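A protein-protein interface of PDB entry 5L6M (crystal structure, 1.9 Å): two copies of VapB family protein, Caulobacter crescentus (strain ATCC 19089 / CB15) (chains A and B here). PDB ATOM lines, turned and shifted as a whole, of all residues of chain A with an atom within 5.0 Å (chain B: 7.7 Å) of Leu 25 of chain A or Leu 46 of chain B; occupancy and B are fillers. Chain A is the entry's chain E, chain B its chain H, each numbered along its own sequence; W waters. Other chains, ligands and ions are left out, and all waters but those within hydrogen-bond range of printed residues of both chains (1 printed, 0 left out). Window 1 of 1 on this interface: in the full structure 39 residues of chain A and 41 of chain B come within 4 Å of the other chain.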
ATOM      1  N   VAL A  23     -25.955 -10.974  27.631  1.00  0.00           N
ATOM      2  CA  VAL A  23     -26.279  -9.589  27.962  1.00  0.00           C
ATOM      3  C   VAL A  23     -27.322  -9.103  26.969  1.00  0.00           C
ATOM      4  O   VAL A  23     -27.210  -9.354  25.764  1.00  0.00           O
ATOM      5  CB  VAL A  23     -25.034  -8.676  27.938  1.00  0.00           C
ATOM      6  CG1 VAL A  23     -25.438  -7.208  28.023  1.00  0.00           C
ATOM      7  CG2 VAL A  23     -24.091  -9.024  29.078  1.00  0.00           C
ATOM      8  N   ARG A  24     -28.342  -8.419  27.479  1.00  0.00           N
ATOM      9  CA  ARG A  24     -29.378  -7.866  26.624  1.00  0.00           C
ATOM     10  C   ARG A  24     -28.930  -6.535  26.032  1.00  0.00           C
ATOM     11  O   ARG A  24     -28.213  -5.754  26.666  1.00  0.00           O
ATOM     12  CB  ARG A  24     -30.687  -7.691  27.398  1.00  0.00           C
ATOM     13  CG  ARG A  24     -31.316  -9.014  27.833  1.00  0.00           C
ATOM     14  CD  ARG A  24     -32.809  -8.880  28.112  1.00  0.00           C
ATOM     15  NE  ARG A  24     -33.444 -10.172  28.376  1.00  0.00           N
ATOM     16  CZ  ARG A  24     -34.760 -10.370  28.361  1.00  0.00           C
ATOM     17  NH1 ARG A  24     -35.578  -9.363  28.085  1.00  0.00           N
ATOM     18  NH2 ARG A  24     -35.261 -11.572  28.614  1.00  0.00           N
ATOM     19  N   LEU A  25     -29.358  -6.291  24.797  1.00  0.00           N
ATOM     20  CA  LEU A  25     -29.031  -5.069  24.065  1.00  0.00           C
ATOM     21  C   LEU A  25     -30.322  -4.331  23.741  1.00  0.00           C
ATOM     22  O   LEU A  25     -31.041  -4.722  22.804  1.00  0.00           O
ATOM     23  CB  LEU A  25     -28.265  -5.398  22.785  1.00  0.00           C
ATOM     24  CG  LEU A  25     -27.076  -6.338  22.978  1.00  0.00           C
ATOM     25  CD1 LEU A  25     -26.414  -6.683  21.650  1.00  0.00           C
ATOM     26  CD2 LEU A  25     -26.074  -5.710  23.942  1.00  0.00           C
ATOM     27  N   PRO A  26     -30.652  -3.258  24.461  1.00  0.00           N
ATOM     28  CA  PRO A  26     -31.895  -2.526  24.186  1.00  0.00           C
ATOM     29  C   PRO A  26     -31.892  -1.934  22.781  1.00  0.00           C
ATOM     30  O   PRO A  26     -30.874  -1.911  22.084  1.00  0.00           O
ATOM     31  CB  PRO A  26     -31.913  -1.433  25.261  1.00  0.00           C
ATOM     32  CG  PRO A  26     -30.881  -1.869  26.272  1.00  0.00           C
ATOM     33  CD  PRO A  26     -29.850  -2.598  25.501  1.00  0.00           C
ATOM     34  N   ARG A  27     -33.062  -1.423  22.382  1.00  0.00           N
ATOM     35  CA  ARG A  27     -33.367  -1.220  20.968  1.00  0.00           C
ATOM     36  C   ARG A  27     -32.269  -0.444  20.241  1.00  0.00           C
ATOM     37  O   ARG A  27     -31.699  -0.922  19.254  1.00  0.00           O
ATOM     38  CB  ARG A  27     -34.716  -0.510  20.832  1.00  0.00           C
ATOM     39  CG  ARG A  27     -35.296  -0.521  19.419  1.00  0.00           C
ATOM     40  CD  ARG A  27     -36.444  -1.506  19.299  1.00  0.00           C
ATOM     41  NE  ARG A  27     -36.046  -2.719  18.591  1.00  0.00           N
ATOM     42  CZ  ARG A  27     -36.822  -3.789  18.440  1.00  0.00           C
ATOM     43  NH1 ARG A  27     -36.374  -4.850  17.778  1.00  0.00           N
ATOM     44  NH2 ARG A  27     -38.043  -3.805  18.957  1.00  0.00           N
ATOM     45  N   LEU A  29     -29.249   0.224  20.853  1.00  0.00           N
ATOM     46  CA  LEU A  29     -27.876  -0.265  20.935  1.00  0.00           C
ATOM     47  C   LEU A  29     -27.675  -1.586  20.203  1.00  0.00           C
ATOM     48  O   LEU A  29     -26.529  -1.974  19.981  1.00  0.00           O
ATOM     49  CB  LEU A  29     -27.441  -0.425  22.407  1.00  0.00           C
ATOM     50  CG  LEU A  29     -27.384   0.838  23.295  1.00  0.00           C
ATOM     51  CD1 LEU A  29     -28.762   1.251  23.828  1.00  0.00           C
ATOM     52  CD2 LEU A  29     -26.404   0.641  24.450  1.00  0.00           C
ATOM     53  N   ALA A  30     -28.753  -2.276  19.825  1.00  0.00           N
ATOM     54  CA  ALA A  30     -28.697  -3.571  19.159  1.00  0.00           C
ATOM     55  C   ALA A  30     -28.322  -3.419  17.690  1.00  0.00           C
ATOM     56  O   ALA A  30     -28.421  -2.336  17.103  1.00  0.00           O
ATOM     57  CB  ALA A  30     -30.047  -4.293  19.279  1.00  0.00           C
ATOM     58  N   PHE A  31     -27.897  -4.541  17.092  1.00  0.00           N
ATOM     59  CA  PHE A  31     -27.435  -4.592  15.710  1.00  0.00           C
ATOM     60  C   PHE A  31     -28.411  -5.283  14.758  1.00  0.00           C
ATOM     61  O   PHE A  31     -28.307  -5.098  13.538  1.00  0.00           O
ATOM     62  CB  PHE A  31     -26.076  -5.317  15.624  1.00  0.00           C
ATOM     63  CG  PHE A  31     -24.903  -4.535  16.219  1.00  0.00           C
ATOM     64  CD1 PHE A  31     -24.178  -3.636  15.441  1.00  0.00           C
ATOM     65  CD2 PHE A  31     -24.509  -4.728  17.536  1.00  0.00           C
ATOM     66  CE1 PHE A  31     -23.095  -2.925  15.979  1.00  0.00           C
ATOM     67  CE2 PHE A  31     -23.432  -4.034  18.074  1.00  0.00           C
ATOM     68  CZ  PHE A  31     -22.725  -3.128  17.291  1.00  0.00           C
ATOM     69  N   LEU A  46     -15.444  -4.685  26.771  1.00  0.00           N
ATOM     70  CA  LEU A  46     -15.856  -5.450  25.608  1.00  0.00           C
ATOM     71  C   LEU A  46     -16.256  -4.491  24.499  1.00  0.00           C
ATOM     72  O   LEU A  46     -17.092  -3.611  24.713  1.00  0.00           O
ATOM     73  CB  LEU A  46     -17.013  -6.370  25.982  1.00  0.00           C
ATOM     74  CG  LEU A  46     -17.580  -7.321  24.932  1.00  0.00           C
ATOM     75  CD1 LEU A  46     -16.526  -8.341  24.516  1.00  0.00           C
ATOM     76  CD2 LEU A  46     -18.776  -8.013  25.533  1.00  0.00           C
ATOM     77  N   THR A  47     -15.662  -4.660  23.323  1.00  0.00           N
ATOM     78  CA  THR A  47     -15.961  -3.838  22.156  1.00  0.00           C
ATOM     79  C   THR A  47     -16.614  -4.699  21.082  1.00  0.00           C
ATOM     80  O   THR A  47     -16.071  -5.746  20.713  1.00  0.00           O
ATOM     81  CB  THR A  47     -14.692  -3.191  21.595  1.00  0.00           C
ATOM     82  OG1 THR A  47     -14.055  -2.398  22.609  1.00  0.00           O
ATOM     83  CG2 THR A  47     -15.038  -2.298  20.399  1.00  0.00           C
ATOM     84  N   ILE A  48     -17.756  -4.249  20.556  1.00  0.00           N
ATOM     85  CA  ILE A  48     -18.533  -5.035  19.603  1.00  0.00           C
ATOM     86  C   ILE A  48     -18.843  -4.179  18.383  1.00  0.00           C
ATOM     87  O   ILE A  48     -19.295  -3.034  18.515  1.00  0.00           O
ATOM     88  CB  ILE A  48     -19.828  -5.577  20.241  1.00  0.00           C
ATOM     89  CG1 ILE A  48     -19.483  -6.345  21.522  1.00  0.00           C
ATOM     90  CG2 ILE A  48     -20.585  -6.458  19.243  1.00  0.00           C
ATOM     91  CD1 ILE A  48     -20.667  -6.657  22.395  1.00  0.00           C
ATOM     92  N   LYS B  13     -23.548 -13.790  16.239  1.00  0.00           N
ATOM     93  CA  LYS B  13     -24.710 -12.958  16.003  1.00  0.00           C
ATOM     94  C   LYS B  13     -25.478 -12.806  17.306  1.00  0.00           C
ATOM     95  O   LYS B  13     -25.286 -13.565  18.260  1.00  0.00           O
ATOM     96  CB  LYS B  13     -25.611 -13.559  14.913  1.00  0.00           C
ATOM     97  CG  LYS B  13     -24.922 -13.720  13.562  1.00  0.00           C
ATOM     98  CD  LYS B  13     -25.914 -14.001  12.437  1.00  0.00           C
ATOM     99  CE  LYS B  13     -25.194 -14.289  11.125  1.00  0.00           C
ATOM    100  NZ  LYS B  13     -26.118 -14.683  10.027  1.00  0.00           N
ATOM    101  N   THR B  14     -26.336 -11.795  17.346  1.00  0.00           N
ATOM    102  CA  THR B  14     -27.235 -11.642  18.472  1.00  0.00           C
ATOM    103  C   THR B  14     -28.336 -12.700  18.397  1.00  0.00           C
ATOM    104  O   THR B  14     -28.390 -13.524  17.478  1.00  0.00           O
ATOM    105  CB  THR B  14     -27.826 -10.237  18.492  1.00  0.00           C
ATOM    106  OG1 THR B  14     -28.684 -10.065  17.358  1.00  0.00           O
ATOM    107  CG2 THR B  14     -26.731  -9.197  18.441  1.00  0.00           C
ATOM    108  N   PHE B  15     -29.219 -12.684  19.389  1.00  0.00           N
ATOM    109  CA  PHE B  15     -30.388 -13.549  19.385  1.00  0.00           C
ATOM    110  C   PHE B  15     -31.493 -12.851  20.162  1.00  0.00           C
ATOM    111  O   PHE B  15     -31.294 -11.773  20.729  1.00  0.00           O
ATOM    112  CB  PHE B  15     -30.063 -14.930  19.954  1.00  0.00           C
ATOM    113  CG  PHE B  15     -29.834 -14.944  21.432  1.00  0.00           C
ATOM    114  CD1 PHE B  15     -28.649 -14.482  21.969  1.00  0.00           C
ATOM    115  CD2 PHE B  15     -30.798 -15.450  22.288  1.00  0.00           C
ATOM    116  CE1 PHE B  15     -28.439 -14.504  23.334  1.00  0.00           C
ATOM    117  CE2 PHE B  15     -30.588 -15.473  23.654  1.00  0.00           C
ATOM    118  CZ  PHE B  15     -29.406 -15.001  24.176  1.00  0.00           C
ATOM    119  N   ASN B  19     -37.624 -11.778  23.261  1.00  0.00           N
ATOM    120  CA  ASN B  19     -37.761 -10.926  22.084  1.00  0.00           C
ATOM    121  C   ASN B  19     -37.127  -9.550  22.279  1.00  0.00           C
ATOM    122  O   ASN B  19     -37.303  -8.656  21.445  1.00  0.00           O
ATOM    123  CB  ASN B  19     -39.232 -10.815  21.669  1.00  0.00           C
ATOM    124  CG  ASN B  19     -39.641 -11.917  20.700  1.00  0.00           C
ATOM    125  OD1 ASN B  19     -39.215 -11.923  19.543  1.00  0.00           O
ATOM    126  ND2 ASN B  19     -40.461 -12.861  21.170  1.00  0.00           N
ATOM    127  N   SER B  20     -36.383  -9.369  23.365  1.00  0.00           N
ATOM    128  CA  SER B  20     -35.330  -8.372  23.393  1.00  0.00           C
ATOM    129  C   SER B  20     -34.071  -8.993  22.809  1.00  0.00           C
ATOM    130  O   SER B  20     -33.833 -10.197  22.942  1.00  0.00           O
ATOM    131  CB  SER B  20     -35.054  -7.873  24.813  1.00  0.00           C
ATOM    132  OG  SER B  20     -33.878  -7.075  24.845  1.00  0.00           O
ATOM    133  N   GLU B  21     -33.271  -8.168  22.145  1.00  0.00           N
ATOM    134  CA  GLU B  21     -32.051  -8.657  21.526  1.00  0.00           C
ATOM    135  C   GLU B  21     -30.981  -8.868  22.591  1.00  0.00           C
ATOM    136  O   GLU B  21     -30.864  -8.089  23.542  1.00  0.00           O
ATOM    137  CB  GLU B  21     -31.563  -7.679  20.453  1.00  0.00           C
ATOM    138  CG  GLU B  21     -30.608  -8.299  19.440  1.00  0.00           C
ATOM    139  CD  GLU B  21     -30.376  -7.427  18.212  1.00  0.00           C
ATOM    140  OE1 GLU B  21     -29.217  -7.015  17.976  1.00  0.00           O
ATOM    141  OE2 GLU B  21     -31.354  -7.152  17.481  1.00  0.00           O
ATOM    142  N   ALA B  22     -30.205  -9.934  22.433  1.00  0.00           N
ATOM    143  CA  ALA B  22     -29.175 -10.275  23.402  1.00  0.00           C
ATOM    144  C   ALA B  22     -27.961 -10.842  22.678  1.00  0.00           C
ATOM    145  O   ALA B  22     -28.059 -11.345  21.557  1.00  0.00           O
ATOM    146  CB  ALA B  22     -29.703 -11.282  24.439  1.00  0.00           C
ATOM    147  N   VAL B  23     -26.814 -10.776  23.344  1.00  0.00           N
ATOM    148  CA  VAL B  23     -25.565 -11.327  22.831  1.00  0.00           C
ATOM    149  C   VAL B  23     -25.067 -12.385  23.808  1.00  0.00           C
ATOM    150  O   VAL B  23     -25.055 -12.154  25.021  1.00  0.00           O
ATOM    151  CB  VAL B  23     -24.512 -10.223  22.610  1.00  0.00           C
ATOM    152  CG1 VAL B  23     -23.124 -10.705  22.982  1.00  0.00           C
ATOM    153  CG2 VAL B  23     -24.525  -9.800  21.167  1.00  0.00           C
ATOM    154  N   ARG B  24     -24.679 -13.547  23.280  1.00  0.00           N
ATOM    155  CA  ARG B  24     -24.093 -14.604  24.094  1.00  0.00           C
ATOM    156  C   ARG B  24     -22.618 -14.318  24.322  1.00  0.00           C
ATOM    157  O   ARG B  24     -21.883 -14.018  23.378  1.00  0.00           O
ATOM    158  CB  ARG B  24     -24.250 -15.968  23.423  1.00  0.00           C
ATOM    159  CG  ARG B  24     -25.672 -16.332  23.045  1.00  0.00           C
ATOM    160  CD  ARG B  24     -25.768 -17.744  22.480  1.00  0.00           C
ATOM    161  NE  ARG B  24     -25.692 -18.767  23.521  1.00  0.00           N
ATOM    162  CZ  ARG B  24     -25.823 -20.070  23.299  1.00  0.00           C
ATOM    163  NH1 ARG B  24     -26.043 -20.517  22.067  1.00  0.00           N
ATOM    164  NH2 ARG B  24     -25.738 -20.931  24.307  1.00  0.00           N
ATOM    165  N   LEU B  25     -22.179 -14.438  25.565  1.00  0.00           N
ATOM    166  CA  LEU B  25     -20.792 -14.156  25.910  1.00  0.00           C
ATOM    167  C   LEU B  25     -20.074 -15.436  26.308  1.00  0.00           C
ATOM    168  O   LEU B  25     -20.392 -16.010  27.361  1.00  0.00           O
ATOM    169  CB  LEU B  25     -20.730 -13.142  27.051  1.00  0.00           C
ATOM    170  CG  LEU B  25     -20.832 -11.652  26.721  1.00  0.00           C
ATOM    171  CD1 LEU B  25     -22.273 -11.200  26.622  1.00  0.00           C
ATOM    172  CD2 LEU B  25     -20.114 -10.893  27.794  1.00  0.00           C
ATOM    173  N   THR B  38     -22.228  -0.985  32.083  1.00  0.00           N
ATOM    174  CA  THR B  38     -22.553   0.188  31.288  1.00  0.00           C
ATOM    175  C   THR B  38     -22.423  -0.182  29.818  1.00  0.00           C
ATOM    176  O   THR B  38     -21.475  -0.869  29.431  1.00  0.00           O
ATOM    177  CB  THR B  38     -21.613   1.354  31.620  1.00  0.00           C
ATOM    178  OG1 THR B  38     -21.875   1.807  32.953  1.00  0.00           O
ATOM    179  CG2 THR B  38     -21.787   2.508  30.624  1.00  0.00           C
ATOM    180  N   LEU B  39     -23.398   0.229  29.012  1.00  0.00           N
ATOM    181  CA  LEU B  39     -23.407  -0.038  27.577  1.00  0.00           C
ATOM    182  C   LEU B  39     -23.516   1.287  26.845  1.00  0.00           C
ATOM    183  O   LEU B  39     -24.345   2.128  27.209  1.00  0.00           O
ATOM    184  CB  LEU B  39     -24.571  -0.945  27.153  1.00  0.00           C
ATOM    185  CG  LEU B  39     -24.792  -2.317  27.815  1.00  0.00           C
ATOM    186  CD1 LEU B  39     -25.545  -2.202  29.136  1.00  0.00           C
ATOM    187  CD2 LEU B  39     -25.536  -3.233  26.865  1.00  0.00           C
ATOM    188  N   ILE B  40     -22.668   1.484  25.838  1.00  0.00           N
ATOM    189  CA  ILE B  40     -22.695   2.712  25.053  1.00  0.00           C
ATOM    190  C   ILE B  40     -22.508   2.335  23.593  1.00  0.00           C
ATOM    191  O   ILE B  40     -21.575   1.607  23.248  1.00  0.00           O
ATOM    192  CB  ILE B  40     -21.648   3.748  25.505  1.00  0.00           C
ATOM    193  CG1 ILE B  40     -21.639   4.946  24.548  1.00  0.00           C
ATOM    194  CG2 ILE B  40     -20.251   3.132  25.631  1.00  0.00           C
ATOM    195  CD1 ILE B  40     -20.738   6.067  24.992  1.00  0.00           C
ATOM    196  N   ARG B  41     -23.421   2.791  22.753  1.00  0.00           N
ATOM    197  CA  ARG B  41     -23.404   2.534  21.325  1.00  0.00           C
ATOM    198  C   ARG B  41     -23.181   3.861  20.605  1.00  0.00           C
ATOM    199  O   ARG B  41     -23.924   4.820  20.841  1.00  0.00           O
ATOM    200  CB  ARG B  41     -24.728   1.908  20.900  1.00  0.00           C
ATOM    201  CG  ARG B  41     -24.878   1.725  19.403  1.00  0.00           C
ATOM    202  CD  ARG B  41     -24.119   0.518  18.888  1.00  0.00           C
ATOM    203  NE  ARG B  41     -24.131   0.513  17.426  1.00  0.00           N
ATOM    204  CZ  ARG B  41     -25.050  -0.095  16.676  1.00  0.00           C
ATOM    205  NH1 ARG B  41     -24.986  -0.008  15.346  1.00  0.00           N
ATOM    206  NH2 ARG B  41     -26.033  -0.785  17.249  1.00  0.00           N
ATOM    207  N   SER B  42     -22.165   3.928  19.736  1.00  0.00           N
ATOM    208  CA  SER B  42     -21.898   5.151  18.962  1.00  0.00           C
ATOM    209  C   SER B  42     -21.531   4.764  17.529  1.00  0.00           C
ATOM    210  O   SER B  42     -20.373   4.488  17.234  1.00  0.00           O
ATOM    211  CB  SER B  42     -20.787   6.005  19.577  1.00  0.00           C
ATOM    212  OG  SER B  42     -21.001   6.237  20.960  1.00  0.00           O
ATOM    213  N   GLY B  43     -22.503   4.793  16.627  1.00  0.00           N
ATOM    214  CA  GLY B  43     -22.177   4.419  15.268  1.00  0.00           C
ATOM    215  C   GLY B  43     -22.013   2.917  15.152  1.00  0.00           C
ATOM    216  O   GLY B  43     -22.933   2.180  15.524  1.00  0.00           O
ATOM    217  N   ASP B  44     -20.855   2.452  14.645  1.00  0.00           N
ATOM    218  CA  ASP B  44     -20.595   1.027  14.480  1.00  0.00           C
ATOM    219  C   ASP B  44     -20.219   0.317  15.773  1.00  0.00           C
ATOM    220  O   ASP B  44     -20.174  -0.920  15.786  1.00  0.00           O
ATOM    221  CB  ASP B  44     -19.456   0.770  13.482  1.00  0.00           C
ATOM    222  CG  ASP B  44     -19.788   1.205  12.079  1.00  0.00           C
ATOM    223  OD1 ASP B  44     -20.985   1.281  11.739  1.00  0.00           O
ATOM    224  OD2 ASP B  44     -18.837   1.457  11.315  1.00  0.00           O
ATOM    225  N   VAL B  45     -19.907   1.035  16.844  1.00  0.00           N
ATOM    226  CA  VAL B  45     -19.258   0.437  18.003  1.00  0.00           C
ATOM    227  C   VAL B  45     -20.207   0.412  19.193  1.00  0.00           C
ATOM    228  O   VAL B  45     -20.766   1.448  19.589  1.00  0.00           O
ATOM    229  CB  VAL B  45     -17.949   1.164  18.341  1.00  0.00           C
ATOM    230  CG1 VAL B  45     -17.294   0.546  19.588  1.00  0.00           C
ATOM    231  CG2 VAL B  45     -17.005   1.084  17.147  1.00  0.00           C
ATOM    232  N   LEU B  46     -20.401  -0.788  19.739  1.00  0.00           N
ATOM    233  CA  LEU B  46     -20.985  -1.002  21.052  1.00  0.00           C
ATOM    234  C   LEU B  46     -19.866  -1.325  22.028  1.00  0.00           C
ATOM    235  O   LEU B  46     -19.030  -2.193  21.753  1.00  0.00           O
ATOM    236  CB  LEU B  46     -21.995  -2.151  21.039  1.00  0.00           C
ATOM    237  CG  LEU B  46     -22.602  -2.507  22.404  1.00  0.00           C
ATOM    238  CD1 LEU B  46     -23.334  -1.319  22.986  1.00  0.00           C
ATOM    239  CD2 LEU B  46     -23.545  -3.699  22.282  1.00  0.00           C
ATOM    240  N   THR B  47     -19.846  -0.626  23.156  1.00  0.00           N
ATOM    241  CA  THR B  47     -18.896  -0.893  24.224  1.00  0.00           C
ATOM    242  C   THR B  47     -19.665  -1.267  25.480  1.00  0.00           C
ATOM    243  O   THR B  47     -20.733  -0.706  25.756  1.00  0.00           O
ATOM    244  CB  THR B  47     -17.992   0.321  24.487  1.00  0.00           C
ATOM    245  OG1 THR B  47     -17.338   0.690  23.264  1.00  0.00           O
ATOM    246  CG2 THR B  47     -16.948  -0.009  25.534  1.00  0.00           C
ATOM    247  N   ILE B  48     -19.149  -2.254  26.214  1.00  0.00           N
ATOM    248  CA  ILE B  48     -19.784  -2.728  27.435  1.00  0.00           C
ATOM    249  C   ILE B  48     -18.706  -2.924  28.490  1.00  0.00           C
ATOM    250  O   ILE B  48     -17.685  -3.570  28.229  1.00  0.00           O
ATOM    251  CB  ILE B  48     -20.563  -4.034  27.202  1.00  0.00           C
ATOM    252  CG1 ILE B  48     -21.673  -3.807  26.170  1.00  0.00           C
ATOM    253  CG2 ILE B  48     -21.133  -4.528  28.517  1.00  0.00           C
ATOM    254  CD1 ILE B  48     -22.356  -5.058  25.698  1.00  0.00           C
HETATM  255  O   HOH W   1     -14.861   0.250  22.984  1.00  0.00           O
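Water W1 lies within hydrogen-bond range of the side-chain hydroxyl (OG1) of Thr 47 of chain B (2.5 Å) and the side-chain hydroxyl (OG1) of Thr 47 of chain A (2.8 Å).
Of chain B, only Glu 21, Val 23, Leu 39 and Leu 46 come within 4 Å of Leu 25 of chain A. Leu 46 of chain B touches just these residues of chain A: Leu 25, Leu 29, Phe 31, Leu 46, Thr 47 and Ile 48. No residue of chain B comes within 4 Å of Pro 26 of chain A. Printed residues of chain A within 4 Å of Thr 47 of chain B: Leu 46 (3.3 Å). Of the printed residues of chain A, Ser 20 of chain B touches Arg 24 (3.6 Å). Of the printed residues of chain A, Glu 21 of chain B touches Arg 24, Leu 25, Ala 30 and Phe 31. Of the printed residues of chain A, Leu 25 of chain B touches Val 23 (3.8 Å) and Leu 46 (3.9 Å). Printed residues of chain A within 4 Å of Leu 39 of chain B: Arg 24, Leu 25 and Leu 29.
OG1 of Thr 14 of chain B sits at hydrogen-bond distance from OE1 of Glu 21 of chain B. The backbone NH (N) of Ala 22 of chain B is in hydrogen-bond range of the backbone carbonyl oxygen (O) of Phe 15 of chain B. The backbone carbonyl oxygen (O) of Ile 40 of chain B is in hydrogen-bond range of the backbone NH (N) of Thr 47 of chain B (2.8 Å). The guanidinium group (NE) of Arg 41 of chain B sits at hydrogen-bond distance from the backbone carbonyl oxygen (O) of Gly 43 of chain B, 2.8 Å away.
Val 23 of chain A touches Leu 25 of chain B, and with the chains exchanged Leu 25 of chain A touches Val 23 of chain B. Leu 25 of chain A touches Leu 46 of chain B, and with the chains exchanged Leu 46 of chain A touches Leu 25 of chain B. Leu 46 of chain B touches its own counterpart, Leu 46 of chain A. Leu 46 of chain A touches Ile 48 of chain B, and with the chains exchanged Ile 48 of chain A touches Leu 46 of chain B. Of the 28 pairs that touch across the chains among the printed residues, 10 have their exchanged pair printed and touching as well.
Of the 21 printed residues of chain B, 12 touch a printed residue of chain A. Along chain B the printed residues that touch a printed residue of chain A span positions 20 to 48. Of the 11 printed residues of chain A, 9 touch a printed residue of chain B. Printed residues of chain A that touch a printed residue of chain B: Val 23, Arg 24, Leu 25, Leu 29, Ala 30, Phe 31, Leu 46, Thr 47 and Ile 48. Hydrophobic or aromatic side chains of chain A within 4 Å of the printed part of chain B: Val 23, Leu 25, Leu 29, Ala 30, Phe 31, Leu 46 and Ile 48. Along chain A the printed residues that touch a printed residue of chain B span positions 23 to 48.
The backbone NH of Val 23 of chain B is in hydrogen-bond range of the backbone carbonyl oxygen of Val 23 of chain A (2.8 Å). N of Leu 25 of chain A is in hydrogen-bond range of O of Glu 21 of chain B (2.7 Å). The backbone carbonyl oxygen (O) of Leu 29 of chain A is in hydrogen-bond range of the guanidinium group (NH2) of Arg 41 of chain B, at 3.0 Å. The backbone carbonyl oxygen of Ala 30 of chain A is in hydrogen-bond range of the guanidinium group of Arg 41 of chain B, 2.9 Å away. The side-chain carboxylate of Glu 21 of chain B is in hydrogen-bond range of the backbone NH of Phe 31 of chain A. O of Leu 46 of chain A sits at hydrogen-bond distance from N of Ile 48 of chain B, at 2.9 Å. N of Ile 48 of chain A lies within hydrogen-bond range of O of Leu 46 of chain B (2.7 Å).
Among the printed residues, pairs that only touch across the chains: Val 23 of chain A with Ala 22 of chain B, Val 23 of chain A with Leu 25 of chain B, Arg 24 of chain A with Ser 20 of chain B, Arg 24 of chain A with Glu 21 of chain B, Arg 24 of chain A with Leu 39 of chain B, Leu 25 of chain A with Val 23 of chain B, Leu 25 of chain A with Leu 39 of chain B, Leu 25 of chain A with Leu 46 of chain B, Leu 29 of chain A with Leu 39 of chain B, Leu 29 of chain A with Leu 46 of chain B, Ala 30 of chain A with Glu 21 of chain B, Phe 31 of chain A with Arg 41 of chain B, Phe 31 of chain A with Asp 44 of chain B, Phe 31 of chain A with Leu 46 of chain B, Leu 46 of chain A with Leu 25 of chain B, Leu 46 of chain A with Leu 46 of chain B, Leu 46 of chain A with Thr 47 of chain B, Thr 47 of chain A with Val 45 of chain B, Thr 47 of chain A with Leu 46 of chain B, Ile 48 of chain A with Asp 44 of chain B and Ile 48 of chain A with Val 45 of chain B.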
